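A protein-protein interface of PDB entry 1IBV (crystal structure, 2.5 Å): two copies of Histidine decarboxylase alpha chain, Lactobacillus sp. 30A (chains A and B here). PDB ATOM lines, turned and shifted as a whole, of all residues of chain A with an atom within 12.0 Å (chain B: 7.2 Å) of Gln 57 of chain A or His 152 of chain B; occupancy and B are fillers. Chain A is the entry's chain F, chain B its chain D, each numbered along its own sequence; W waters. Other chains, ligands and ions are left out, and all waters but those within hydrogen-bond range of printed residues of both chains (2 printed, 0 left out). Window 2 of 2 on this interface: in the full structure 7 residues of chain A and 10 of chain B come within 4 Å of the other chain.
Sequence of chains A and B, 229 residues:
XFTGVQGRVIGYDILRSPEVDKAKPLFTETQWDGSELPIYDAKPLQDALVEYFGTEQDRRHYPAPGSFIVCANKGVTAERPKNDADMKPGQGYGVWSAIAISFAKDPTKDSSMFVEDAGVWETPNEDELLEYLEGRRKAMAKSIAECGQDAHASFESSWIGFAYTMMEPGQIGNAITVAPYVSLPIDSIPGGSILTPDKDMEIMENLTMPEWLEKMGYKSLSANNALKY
Among the printed residues, pairs that only touch across the chains: Glu 56 of chain A with Asp 150 of chain B, Glu 56 of chain A with Ala 151 of chain B and Pro 65 of chain A with Lys 109 of chain B.
Gln 57 of chain A touches just one residue of chain B: His 152.
Of chain A, only Glu 56 and Gln 57 come within 4 Å of His 152 of chain B.
No residue of chain A comes within 4 Å of Trp 32 of chain B.
No residue of chain A comes within 4 Å of Gly 148 of chain B.
No residue of chain A comes within 4 Å of Gln 149 of chain B.
Of chain A, only Glu 56 comes within 4 Å of Asp 150 of chain B.
Of chain A, only Glu 56 and Arg 59 come within 4 Å of Ala 151 of chain B.
No residue of chain A comes within 4 Å of Ala 153 of chain B.
Of the printed residues of chain B, Arg 59 of chain A touches Ala 151 (2.7 Å).
Of the printed residues of chain B, Glu 56 of chain A touches Asp 150, Ala 151 and His 152.
Printed residues of chain B within 4 Å of Pro 65 of chain A: Lys 109.
Lys 219 of chain A touches none of the printed residues of chain B.
Leu 227 of chain A touches none of the printed residues of chain B.
The nearest residue of chain B that does not touch Gln 57 of chain A is Asp 150 of chain B (6.4 Å).
Hydrophobic or aromatic side chains of chain A within 4 Å of the printed part of chain B: Pro 65.
Printed residues of chain B that touch a printed residue of chain A: Lys 109, Asp 150, Ala 151 and His 152.
Hydrophobic or aromatic side chains of chain B that line the printed part of chain A: His 152.
Among the printed residues, 6 pairs touch across the chains.
Among the printed residues, no Asp or Glu carboxylate lies within 4 Å of a Lys or Arg side-chain nitrogen of the other chain.
NE2 of His 152 of chain B lies close to OE1 of Glu 56 of chain A, 3.2 Å away.
O of Ala 151 of chain B sits at hydrogen-bond distance from NH1 of Arg 59 of chain A, 2.7 Å away.
The side-chain amide oxygen of Gln 57 of chain A sits close to a ring nitrogen (NE2) of His 152 of chain B, at 3.3 Å.
Water W1 lies within hydrogen-bond range of NH2 of Arg 59 of chain A (2.7 Å), O of Ala 151 of chain B (3.0 Å) and OD1 of Asp 110 of chain B (3.1 Å).
Water W2 lies within hydrogen-bond range of OH of Tyr 62 of chain A (2.8 Å), O of Lys 109 of chain B (2.8 Å) and NH2 of Arg 59 of chain A (3.1 Å).
No position is printed for both chains.
Of the 6 pairs that touch across the chains among the printed residues, none has its exchanged pair printed and touching as well.
NE2 of Gln 57 of chain A sits at hydrogen-bond distance from OE1 of Glu 56 of chain A (2.8 Å).
The side-chain carboxylate (OE2) of Glu 56 of chain A is in salt-bridge range of the guanidinium group (NH1) of Arg 59 of chain A (2.8 Å).
O of Gln 149 of chain B sits at hydrogen-bond distance from ND1 of His 152 of chain B (3.0 Å).
NZ of Lys 109 of chain B is in salt-bridge range of OD2 of Asp 110 of chain B, 3.9 Å away.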
ATOM      1  N   VAL A  50      -0.225  -7.569   9.623  1.00  0.00           N
ATOM      2  CA  VAL A  50      -1.419  -6.831  10.008  1.00  0.00           C
ATOM      3  C   VAL A  50      -2.660  -7.613   9.599  1.00  0.00           C
ATOM      4  O   VAL A  50      -3.648  -7.654  10.325  1.00  0.00           O
ATOM      5  CB  VAL A  50      -1.450  -5.435   9.367  1.00  0.00           C
ATOM      6  CG1 VAL A  50      -2.656  -4.639   9.872  1.00  0.00           C
ATOM      7  CG2 VAL A  50      -0.164  -4.691   9.683  1.00  0.00           C
ATOM      8  N   GLU A  51      -2.596  -8.257   8.445  1.00  0.00           N
ATOM      9  CA  GLU A  51      -3.720  -9.034   7.957  1.00  0.00           C
ATOM     10  C   GLU A  51      -4.049 -10.209   8.877  1.00  0.00           C
ATOM     11  O   GLU A  51      -5.212 -10.576   9.031  1.00  0.00           O
ATOM     12  CB  GLU A  51      -3.431  -9.538   6.541  1.00  0.00           C
ATOM     13  CG  GLU A  51      -3.277  -8.440   5.498  1.00  0.00           C
ATOM     14  CD  GLU A  51      -4.602  -7.824   5.080  1.00  0.00           C
ATOM     15  OE1 GLU A  51      -5.542  -7.776   5.903  1.00  0.00           O
ATOM     16  OE2 GLU A  51      -4.709  -7.390   3.916  1.00  0.00           O
ATOM     17  N   TYR A  52      -3.017 -10.800   9.477  1.00  0.00           N
ATOM     18  CA  TYR A  52      -3.194 -11.949  10.369  1.00  0.00           C
ATOM     19  C   TYR A  52      -3.580 -11.545  11.796  1.00  0.00           C
ATOM     20  O   TYR A  52      -4.565 -12.052  12.340  1.00  0.00           O
ATOM     21  CB  TYR A  52      -1.929 -12.813  10.389  1.00  0.00           C
ATOM     22  CG  TYR A  52      -2.124 -14.155  11.058  1.00  0.00           C
ATOM     23  CD1 TYR A  52      -2.892 -15.144  10.454  1.00  0.00           C
ATOM     24  CD2 TYR A  52      -1.567 -14.418  12.307  1.00  0.00           C
ATOM     25  CE1 TYR A  52      -3.108 -16.359  11.074  1.00  0.00           C
ATOM     26  CE2 TYR A  52      -1.775 -15.626  12.935  1.00  0.00           C
ATOM     27  CZ  TYR A  52      -2.549 -16.593  12.313  1.00  0.00           C
ATOM     28  OH  TYR A  52      -2.783 -17.791  12.936  1.00  0.00           O
ATOM     29  N   PHE A  53      -2.793 -10.668  12.414  1.00  0.00           N
ATOM     30  CA  PHE A  53      -3.092 -10.211  13.768  1.00  0.00           C
ATOM     31  C   PHE A  53      -4.312  -9.314  13.830  1.00  0.00           C
ATOM     32  O   PHE A  53      -5.051  -9.328  14.810  1.00  0.00           O
ATOM     33  CB  PHE A  53      -1.912  -9.451  14.364  1.00  0.00           C
ATOM     34  CG  PHE A  53      -0.796 -10.329  14.839  1.00  0.00           C
ATOM     35  CD1 PHE A  53       0.320  -9.773  15.448  1.00  0.00           C
ATOM     36  CD2 PHE A  53      -0.857 -11.707  14.685  1.00  0.00           C
ATOM     37  CE1 PHE A  53       1.368 -10.568  15.880  1.00  0.00           C
ATOM     38  CE2 PHE A  53       0.187 -12.518  15.113  1.00  0.00           C
ATOM     39  CZ  PHE A  53       1.300 -11.948  15.718  1.00  0.00           C
ATOM     40  N   GLY A  54      -4.549  -8.566  12.764  1.00  0.00           N
ATOM     41  CA  GLY A  54      -5.663  -7.646  12.759  1.00  0.00           C
ATOM     42  C   GLY A  54      -5.181  -6.379  13.444  1.00  0.00           C
ATOM     43  O   GLY A  54      -4.021  -6.297  13.876  1.00  0.00           O
ATOM     44  N   THR A  55      -6.059  -5.396  13.559  1.00  0.00           N
ATOM     45  CA  THR A  55      -5.712  -4.128  14.184  1.00  0.00           C
ATOM     46  C   THR A  55      -6.467  -3.971  15.487  1.00  0.00           C
ATOM     47  O   THR A  55      -7.378  -4.736  15.775  1.00  0.00           O
ATOM     48  CB  THR A  55      -6.066  -2.948  13.268  1.00  0.00           C
ATOM     49  OG1 THR A  55      -7.470  -2.966  12.973  1.00  0.00           O
ATOM     50  CG2 THR A  55      -5.271  -3.029  11.968  1.00  0.00           C
ATOM     51  N   GLU A  56      -6.167  -2.907  16.214  1.00  0.00           N
ATOM     52  CA  GLU A  56      -6.818  -2.668  17.491  1.00  0.00           C
ATOM     53  C   GLU A  56      -8.337  -2.595  17.397  1.00  0.00           C
ATOM     54  O   GLU A  56      -9.035  -3.029  18.309  1.00  0.00           O
ATOM     55  CB  GLU A  56      -6.259  -1.401  18.128  1.00  0.00           C
ATOM     56  CG  GLU A  56      -6.490  -1.303  19.634  1.00  0.00           C
ATOM     57  CD  GLU A  56      -7.915  -0.954  19.996  1.00  0.00           C
ATOM     58  OE1 GLU A  56      -8.343   0.165  19.639  1.00  0.00           O
ATOM     59  OE2 GLU A  56      -8.609  -1.792  20.620  1.00  0.00           O
ATOM     60  N   GLN A  57      -8.862  -2.051  16.309  1.00  0.00           N
ATOM     61  CA  GLN A  57     -10.310  -1.959  16.178  1.00  0.00           C
ATOM     62  C   GLN A  57     -10.891  -3.109  15.387  1.00  0.00           C
ATOM     63  O   GLN A  57     -12.090  -3.370  15.445  1.00  0.00           O
ATOM     64  CB  GLN A  57     -10.723  -0.643  15.521  1.00  0.00           C
ATOM     65  CG  GLN A  57     -11.758   0.126  16.315  1.00  0.00           C
ATOM     66  CD  GLN A  57     -11.171   0.682  17.589  1.00  0.00           C
ATOM     67  OE1 GLN A  57     -11.819   0.709  18.640  1.00  0.00           O
ATOM     68  NE2 GLN A  57      -9.924   1.130  17.507  1.00  0.00           N
ATOM     69  N   ASP A  58     -10.035  -3.777  14.626  1.00  0.00           N
ATOM     70  CA  ASP A  58     -10.455  -4.897  13.800  1.00  0.00           C
ATOM     71  C   ASP A  58      -9.509  -6.059  14.108  1.00  0.00           C
ATOM     72  O   ASP A  58      -8.688  -6.462  13.279  1.00  0.00           O
ATOM     73  CB  ASP A  58     -10.379  -4.501  12.325  1.00  0.00           C
ATOM     74  CG  ASP A  58     -11.148  -5.438  11.433  1.00  0.00           C
ATOM     75  OD1 ASP A  58     -11.315  -6.614  11.816  1.00  0.00           O
ATOM     76  OD2 ASP A  58     -11.593  -5.002  10.350  1.00  0.00           O
ATOM     77  N   ARG A  59      -9.643  -6.583  15.321  1.00  0.00           N
ATOM     78  CA  ARG A  59      -8.812  -7.668  15.833  1.00  0.00           C
ATOM     79  C   ARG A  59      -9.083  -9.034  15.229  1.00  0.00           C
ATOM     80  O   ARG A  59     -10.232  -9.461  15.094  1.00  0.00           O
ATOM     81  CB  ARG A  59      -8.939  -7.752  17.350  1.00  0.00           C
ATOM     82  CG  ARG A  59      -8.552  -6.484  18.066  1.00  0.00           C
ATOM     83  CD  ARG A  59      -8.628  -6.663  19.552  1.00  0.00           C
ATOM     84  NE  ARG A  59      -8.440  -5.397  20.240  1.00  0.00           N
ATOM     85  CZ  ARG A  59      -8.239  -5.284  21.543  1.00  0.00           C
ATOM     86  NH1 ARG A  59      -8.081  -4.091  22.097  1.00  0.00           N
ATOM     87  NH2 ARG A  59      -8.167  -6.371  22.291  1.00  0.00           N
ATOM     88  N   ARG A  60      -8.000  -9.732  14.901  1.00  0.00           N
ATOM     89  CA  ARG A  60      -8.090 -11.053  14.323  1.00  0.00           C
ATOM     90  C   ARG A  60      -7.330 -12.056  15.182  1.00  0.00           C
ATOM     91  O   ARG A  60      -7.711 -12.297  16.323  1.00  0.00           O
ATOM     92  CB  ARG A  60      -7.595 -11.036  12.878  1.00  0.00           C
ATOM     93  CG  ARG A  60      -8.511 -10.236  11.987  1.00  0.00           C
ATOM     94  CD  ARG A  60      -7.932  -9.992  10.619  1.00  0.00           C
ATOM     95  NE  ARG A  60      -8.878  -9.230   9.811  1.00  0.00           N
ATOM     96  CZ  ARG A  60      -8.645  -8.803   8.577  1.00  0.00           C
ATOM     97  NH1 ARG A  60      -9.582  -8.119   7.936  1.00  0.00           N
ATOM     98  NH2 ARG A  60      -7.490  -9.062   7.986  1.00  0.00           N
ATOM     99  N   HIS A  61      -6.240 -12.607  14.673  1.00  0.00           N
ATOM    100  CA  HIS A  61      -5.490 -13.595  15.432  1.00  0.00           C
ATOM    101  C   HIS A  61      -4.302 -13.034  16.173  1.00  0.00           C
ATOM    102  O   HIS A  61      -3.175 -13.506  16.043  1.00  0.00           O
ATOM    103  CB  HIS A  61      -5.132 -14.753  14.513  1.00  0.00           C
ATOM    104  CG  HIS A  61      -6.322 -15.302  13.804  1.00  0.00           C
ATOM    105  ND1 HIS A  61      -7.314 -16.000  14.460  1.00  0.00           N
ATOM    106  CD2 HIS A  61      -6.749 -15.159  12.528  1.00  0.00           C
ATOM    107  CE1 HIS A  61      -8.303 -16.254  13.624  1.00  0.00           C
ATOM    108  NE2 HIS A  61      -7.985 -15.755  12.441  1.00  0.00           N
ATOM    109  N   TYR A  62      -4.567 -12.006  16.965  1.00  0.00           N
ATOM    110  CA  TYR A  62      -3.526 -11.366  17.743  1.00  0.00           C
ATOM    111  C   TYR A  62      -3.146 -12.268  18.902  1.00  0.00           C
ATOM    112  O   TYR A  62      -3.879 -13.188  19.248  1.00  0.00           O
ATOM    113  CB  TYR A  62      -4.018 -10.010  18.251  1.00  0.00           C
ATOM    114  CG  TYR A  62      -5.157 -10.080  19.234  1.00  0.00           C
ATOM    115  CD1 TYR A  62      -6.465 -10.267  18.799  1.00  0.00           C
ATOM    116  CD2 TYR A  62      -4.926  -9.928  20.600  1.00  0.00           C
ATOM    117  CE1 TYR A  62      -7.513 -10.296  19.702  1.00  0.00           C
ATOM    118  CE2 TYR A  62      -5.962  -9.953  21.507  1.00  0.00           C
ATOM    119  CZ  TYR A  62      -7.253 -10.136  21.053  1.00  0.00           C
ATOM    120  OH  TYR A  62      -8.286 -10.160  21.952  1.00  0.00           O
ATOM    121  N   PRO A  65      -4.177 -12.439  25.416  1.00  0.00           N
ATOM    122  CA  PRO A  65      -4.045 -11.432  26.467  1.00  0.00           C
ATOM    123  C   PRO A  65      -3.215 -11.937  27.631  1.00  0.00           C
ATOM    124  O   PRO A  65      -3.635 -12.844  28.354  1.00  0.00           O
ATOM    125  CB  PRO A  65      -5.489 -11.202  26.894  1.00  0.00           C
ATOM    126  CG  PRO A  65      -6.238 -11.425  25.634  1.00  0.00           C
ATOM    127  CD  PRO A  65      -5.593 -12.663  25.090  1.00  0.00           C
ATOM    128  N   TYR A 218     -12.490 -12.321   5.612  1.00  0.00           N
ATOM    129  CA  TYR A 218     -11.813 -11.124   6.091  1.00  0.00           C
ATOM    130  C   TYR A 218     -11.590 -10.159   4.944  1.00  0.00           C
ATOM    131  O   TYR A 218     -11.272 -10.575   3.827  1.00  0.00           O
ATOM    132  CB  TYR A 218     -10.449 -11.476   6.687  1.00  0.00           C
ATOM    133  CG  TYR A 218     -10.505 -12.209   8.008  1.00  0.00           C
ATOM    134  CD1 TYR A 218     -11.672 -12.233   8.766  1.00  0.00           C
ATOM    135  CD2 TYR A 218      -9.383 -12.872   8.497  1.00  0.00           C
ATOM    136  CE1 TYR A 218     -11.717 -12.903   9.981  1.00  0.00           C
ATOM    137  CE2 TYR A 218      -9.417 -13.541   9.705  1.00  0.00           C
ATOM    138  CZ  TYR A 218     -10.584 -13.554  10.446  1.00  0.00           C
ATOM    139  OH  TYR A 218     -10.609 -14.208  11.659  1.00  0.00           O
ATOM    140  N   LYS A 219     -11.793  -8.877   5.210  1.00  0.00           N
ATOM    141  CA  LYS A 219     -11.559  -7.862   4.194  1.00  0.00           C
ATOM    142  C   LYS A 219     -10.049  -7.675   4.211  1.00  0.00           C
ATOM    143  O   LYS A 219      -9.389  -8.101   5.155  1.00  0.00           O
ATOM    144  CB  LYS A 219     -12.242  -6.538   4.557  1.00  0.00           C
ATOM    145  CG  LYS A 219     -13.281  -6.611   5.685  1.00  0.00           C
ATOM    146  CD  LYS A 219     -12.611  -6.561   7.069  1.00  0.00           C
ATOM    147  CE  LYS A 219     -13.513  -7.147   8.143  1.00  0.00           C
ATOM    148  NZ  LYS A 219     -13.810  -8.588   7.862  1.00  0.00           N
ATOM    149  N   LEU A 221      -6.959  -5.588   4.912  1.00  0.00           N
ATOM    150  CA  LEU A 221      -6.569  -4.392   5.637  1.00  0.00           C
ATOM    151  C   LEU A 221      -5.439  -3.657   4.924  1.00  0.00           C
ATOM    152  O   LEU A 221      -5.306  -2.445   5.065  1.00  0.00           O
ATOM    153  CB  LEU A 221      -6.155  -4.741   7.065  1.00  0.00           C
ATOM    154  CG  LEU A 221      -7.304  -5.201   7.965  1.00  0.00           C
ATOM    155  CD1 LEU A 221      -6.751  -5.733   9.264  1.00  0.00           C
ATOM    156  CD2 LEU A 221      -8.275  -4.058   8.231  1.00  0.00           C
ATOM    157  N   LEU A 227      -1.897   0.791   4.490  1.00  0.00           N
ATOM    158  CA  LEU A 227      -1.130   0.734   5.733  1.00  0.00           C
ATOM    159  C   LEU A 227       0.154   1.543   5.666  1.00  0.00           C
ATOM    160  O   LEU A 227       0.923   1.411   4.722  1.00  0.00           O
ATOM    161  CB  LEU A 227      -0.803  -0.722   6.080  1.00  0.00           C
ATOM    162  CG  LEU A 227      -1.727  -1.537   6.997  1.00  0.00           C
ATOM    163  CD1 LEU A 227      -3.088  -0.890   7.210  1.00  0.00           C
ATOM    164  CD2 LEU A 227      -1.882  -2.912   6.408  1.00  0.00           C
ATOM    165  N   TRP B  32     -11.100   5.662  29.765  1.00  0.00           N
ATOM    166  CA  TRP B  32     -11.678   5.951  28.460  1.00  0.00           C
ATOM    167  C   TRP B  32     -13.189   5.796  28.376  1.00  0.00           C
ATOM    168  O   TRP B  32     -13.827   6.460  27.564  1.00  0.00           O
ATOM    169  CB  TRP B  32     -11.021   5.077  27.386  1.00  0.00           C
ATOM    170  CG  TRP B  32     -11.411   3.633  27.457  1.00  0.00           C
ATOM    171  CD1 TRP B  32     -10.852   2.669  28.244  1.00  0.00           C
ATOM    172  CD2 TRP B  32     -12.467   2.990  26.726  1.00  0.00           C
ATOM    173  NE1 TRP B  32     -11.496   1.471  28.058  1.00  0.00           N
ATOM    174  CE2 TRP B  32     -12.487   1.638  27.129  1.00  0.00           C
ATOM    175  CE3 TRP B  32     -13.396   3.425  25.766  1.00  0.00           C
ATOM    176  CZ2 TRP B  32     -13.404   0.718  26.617  1.00  0.00           C
ATOM    177  CZ3 TRP B  32     -14.308   2.508  25.255  1.00  0.00           C
ATOM    178  CH2 TRP B  32     -14.301   1.171  25.679  1.00  0.00           C
ATOM    179  N   LYS B 109     -11.673 -11.104  28.138  1.00  0.00           N
ATOM    180  CA  LYS B 109     -11.423 -10.326  26.929  1.00  0.00           C
ATOM    181  C   LYS B 109     -10.174  -9.485  27.079  1.00  0.00           C
ATOM    182  O   LYS B 109      -9.326  -9.454  26.187  1.00  0.00           O
ATOM    183  CB  LYS B 109     -12.590  -9.389  26.608  1.00  0.00           C
ATOM    184  CG  LYS B 109     -13.749 -10.002  25.835  1.00  0.00           C
ATOM    185  CD  LYS B 109     -14.616  -8.899  25.221  1.00  0.00           C
ATOM    186  CE  LYS B 109     -15.006  -7.817  26.261  1.00  0.00           C
ATOM    187  NZ  LYS B 109     -14.452  -6.440  25.999  1.00  0.00           N
ATOM    188  N   ASP B 110     -10.067  -8.793  28.204  1.00  0.00           N
ATOM    189  CA  ASP B 110      -8.928  -7.915  28.451  1.00  0.00           C
ATOM    190  C   ASP B 110      -7.977  -8.469  29.509  1.00  0.00           C
ATOM    191  O   ASP B 110      -8.410  -9.117  30.465  1.00  0.00           O
ATOM    192  CB  ASP B 110      -9.426  -6.526  28.891  1.00  0.00           C
ATOM    193  CG  ASP B 110     -10.420  -5.918  27.913  1.00  0.00           C
ATOM    194  OD1 ASP B 110     -10.143  -5.928  26.697  1.00  0.00           O
ATOM    195  OD2 ASP B 110     -11.479  -5.428  28.363  1.00  0.00           O
ATOM    196  N   GLU B 146      -4.095   5.755  30.322  1.00  0.00           N
ATOM    197  CA  GLU B 146      -3.634   5.998  28.967  1.00  0.00           C
ATOM    198  C   GLU B 146      -3.414   4.683  28.236  1.00  0.00           C
ATOM    199  O   GLU B 146      -3.814   4.543  27.075  1.00  0.00           O
ATOM    200  CB  GLU B 146      -2.357   6.822  28.977  1.00  0.00           C
ATOM    201  CG  GLU B 146      -2.546   8.214  28.424  1.00  0.00           C
ATOM    202  CD  GLU B 146      -1.434   9.154  28.819  1.00  0.00           C
ATOM    203  OE1 GLU B 146      -0.252   8.758  28.756  1.00  0.00           O
ATOM    204  OE2 GLU B 146      -1.746  10.299  29.197  1.00  0.00           O
ATOM    205  N   CYS B 147      -2.816   3.707  28.917  1.00  0.00           N
ATOM    206  CA  CYS B 147      -2.578   2.413  28.297  1.00  0.00           C
ATOM    207  C   CYS B 147      -3.900   1.704  28.043  1.00  0.00           C
ATOM    208  O   CYS B 147      -4.099   1.102  26.986  1.00  0.00           O
ATOM    209  CB  CYS B 147      -1.659   1.554  29.156  1.00  0.00           C
ATOM    210  SG  CYS B 147       0.107   1.903  28.924  1.00  0.00           S
ATOM    211  N   GLY B 148      -4.822   1.818  28.992  1.00  0.00           N
ATOM    212  CA  GLY B 148      -6.122   1.196  28.831  1.00  0.00           C
ATOM    213  C   GLY B 148      -6.738   1.737  27.562  1.00  0.00           C
ATOM    214  O   GLY B 148      -7.288   0.998  26.748  1.00  0.00           O
ATOM    215  N   GLN B 149      -6.599   3.045  27.391  1.00  0.00           N
ATOM    216  CA  GLN B 149      -7.095   3.762  26.225  1.00  0.00           C
ATOM    217  C   GLN B 149      -6.640   3.054  24.946  1.00  0.00           C
ATOM    218  O   GLN B 149      -7.457   2.721  24.081  1.00  0.00           O
ATOM    219  CB  GLN B 149      -6.553   5.203  26.257  1.00  0.00           C
ATOM    220  CG  GLN B 149      -6.915   6.066  25.073  1.00  0.00           C
ATOM    221  CD  GLN B 149      -8.404   6.282  24.973  1.00  0.00           C
ATOM    222  OE1 GLN B 149      -9.118   5.468  24.392  1.00  0.00           O
ATOM    223  NE2 GLN B 149      -8.891   7.368  25.570  1.00  0.00           N
ATOM    224  N   ASP B 150      -5.342   2.776  24.874  1.00  0.00           N
ATOM    225  CA  ASP B 150      -4.754   2.124  23.715  1.00  0.00           C
ATOM    226  C   ASP B 150      -5.389   0.798  23.324  1.00  0.00           C
ATOM    227  O   ASP B 150      -5.501   0.490  22.141  1.00  0.00           O
ATOM    228  CB  ASP B 150      -3.253   1.919  23.934  1.00  0.00           C
ATOM    229  CG  ASP B 150      -2.503   3.227  24.128  1.00  0.00           C
ATOM    230  OD1 ASP B 150      -1.359   3.185  24.634  1.00  0.00           O
ATOM    231  OD2 ASP B 150      -3.049   4.299  23.770  1.00  0.00           O
ATOM    232  N   ALA B 151      -5.789   0.007  24.313  1.00  0.00           N
ATOM    233  CA  ALA B 151      -6.388  -1.297  24.032  1.00  0.00           C
ATOM    234  C   ALA B 151      -7.856  -1.366  24.378  1.00  0.00           C
ATOM    235  O   ALA B 151      -8.489  -2.398  24.197  1.00  0.00           O
ATOM    236  CB  ALA B 151      -5.628  -2.395  24.775  1.00  0.00           C
ATOM    237  N   HIS B 152      -8.408  -0.253  24.842  1.00  0.00           N
ATOM    238  CA  HIS B 152      -9.811  -0.210  25.238  1.00  0.00           C
ATOM    239  C   HIS B 152     -10.052  -1.310  26.275  1.00  0.00           C
ATOM    240  O   HIS B 152     -10.983  -2.121  26.167  1.00  0.00           O
ATOM    241  CB  HIS B 152     -10.722  -0.361  24.015  1.00  0.00           C
ATOM    242  CG  HIS B 152     -10.577   0.741  23.022  1.00  0.00           C
ATOM    243  ND1 HIS B 152     -10.351   2.057  23.392  1.00  0.00           N
ATOM    244  CD2 HIS B 152     -10.574   0.740  21.668  1.00  0.00           C
ATOM    245  CE1 HIS B 152     -10.211   2.801  22.318  1.00  0.00           C
ATOM    246  NE2 HIS B 152     -10.343   2.023  21.251  1.00  0.00           N
ATOM    247  N   ALA B 153      -9.174  -1.330  27.277  1.00  0.00           N
ATOM    248  CA  ALA B 153      -9.231  -2.305  28.349  1.00  0.00           C
ATOM    249  C   ALA B 153      -9.608  -1.597  29.625  1.00  0.00           C
ATOM    250  O   ALA B 153      -8.820  -0.829  30.159  1.00  0.00           O
ATOM    251  CB  ALA B 153      -7.893  -2.961  28.509  1.00  0.00           C
ATOM    252  N   SER B 154     -10.813  -1.837  30.109  1.00  0.00           N
ATOM    253  CA  SER B 154     -11.271  -1.214  31.336  1.00  0.00           C
ATOM    254  C   SER B 154     -10.913  -2.054  32.550  1.00  0.00           C
ATOM    255  O   SER B 154     -11.092  -3.273  32.555  1.00  0.00           O
ATOM    256  CB  SER B 154     -12.774  -0.981  31.268  1.00  0.00           C
ATOM    257  OG  SER B 154     -13.095  -0.250  30.095  1.00  0.00           O
ATOM    258  N   PHE B 155     -10.391  -1.389  33.567  1.00  0.00           N
ATOM    259  CA  PHE B 155      -9.988  -2.032  34.802  1.00  0.00           C
ATOM    260  C   PHE B 155     -10.997  -1.694  35.885  1.00  0.00           C
ATOM    261  O   PHE B 155     -11.756  -0.736  35.763  1.00  0.00           O
ATOM    262  CB  PHE B 155      -8.593  -1.556  35.206  1.00  0.00           C
ATOM    263  CG  PHE B 155      -7.596  -1.613  34.084  1.00  0.00           C
ATOM    264  CD1 PHE B 155      -7.163  -2.835  33.591  1.00  0.00           C
ATOM    265  CD2 PHE B 155      -7.131  -0.448  33.480  1.00  0.00           C
ATOM    266  CE1 PHE B 155      -6.291  -2.898  32.507  1.00  0.00           C
ATOM    267  CE2 PHE B 155      -6.256  -0.504  32.390  1.00  0.00           C
ATOM    268  CZ  PHE B 155      -5.837  -1.731  31.909  1.00  0.00           C
HETATM  269  O   HOH W   1      -7.785  -5.213  24.754  1.00  0.00           O
HETATM  270  O   HOH W   2      -7.468  -8.684  24.194  1.00  0.00           O
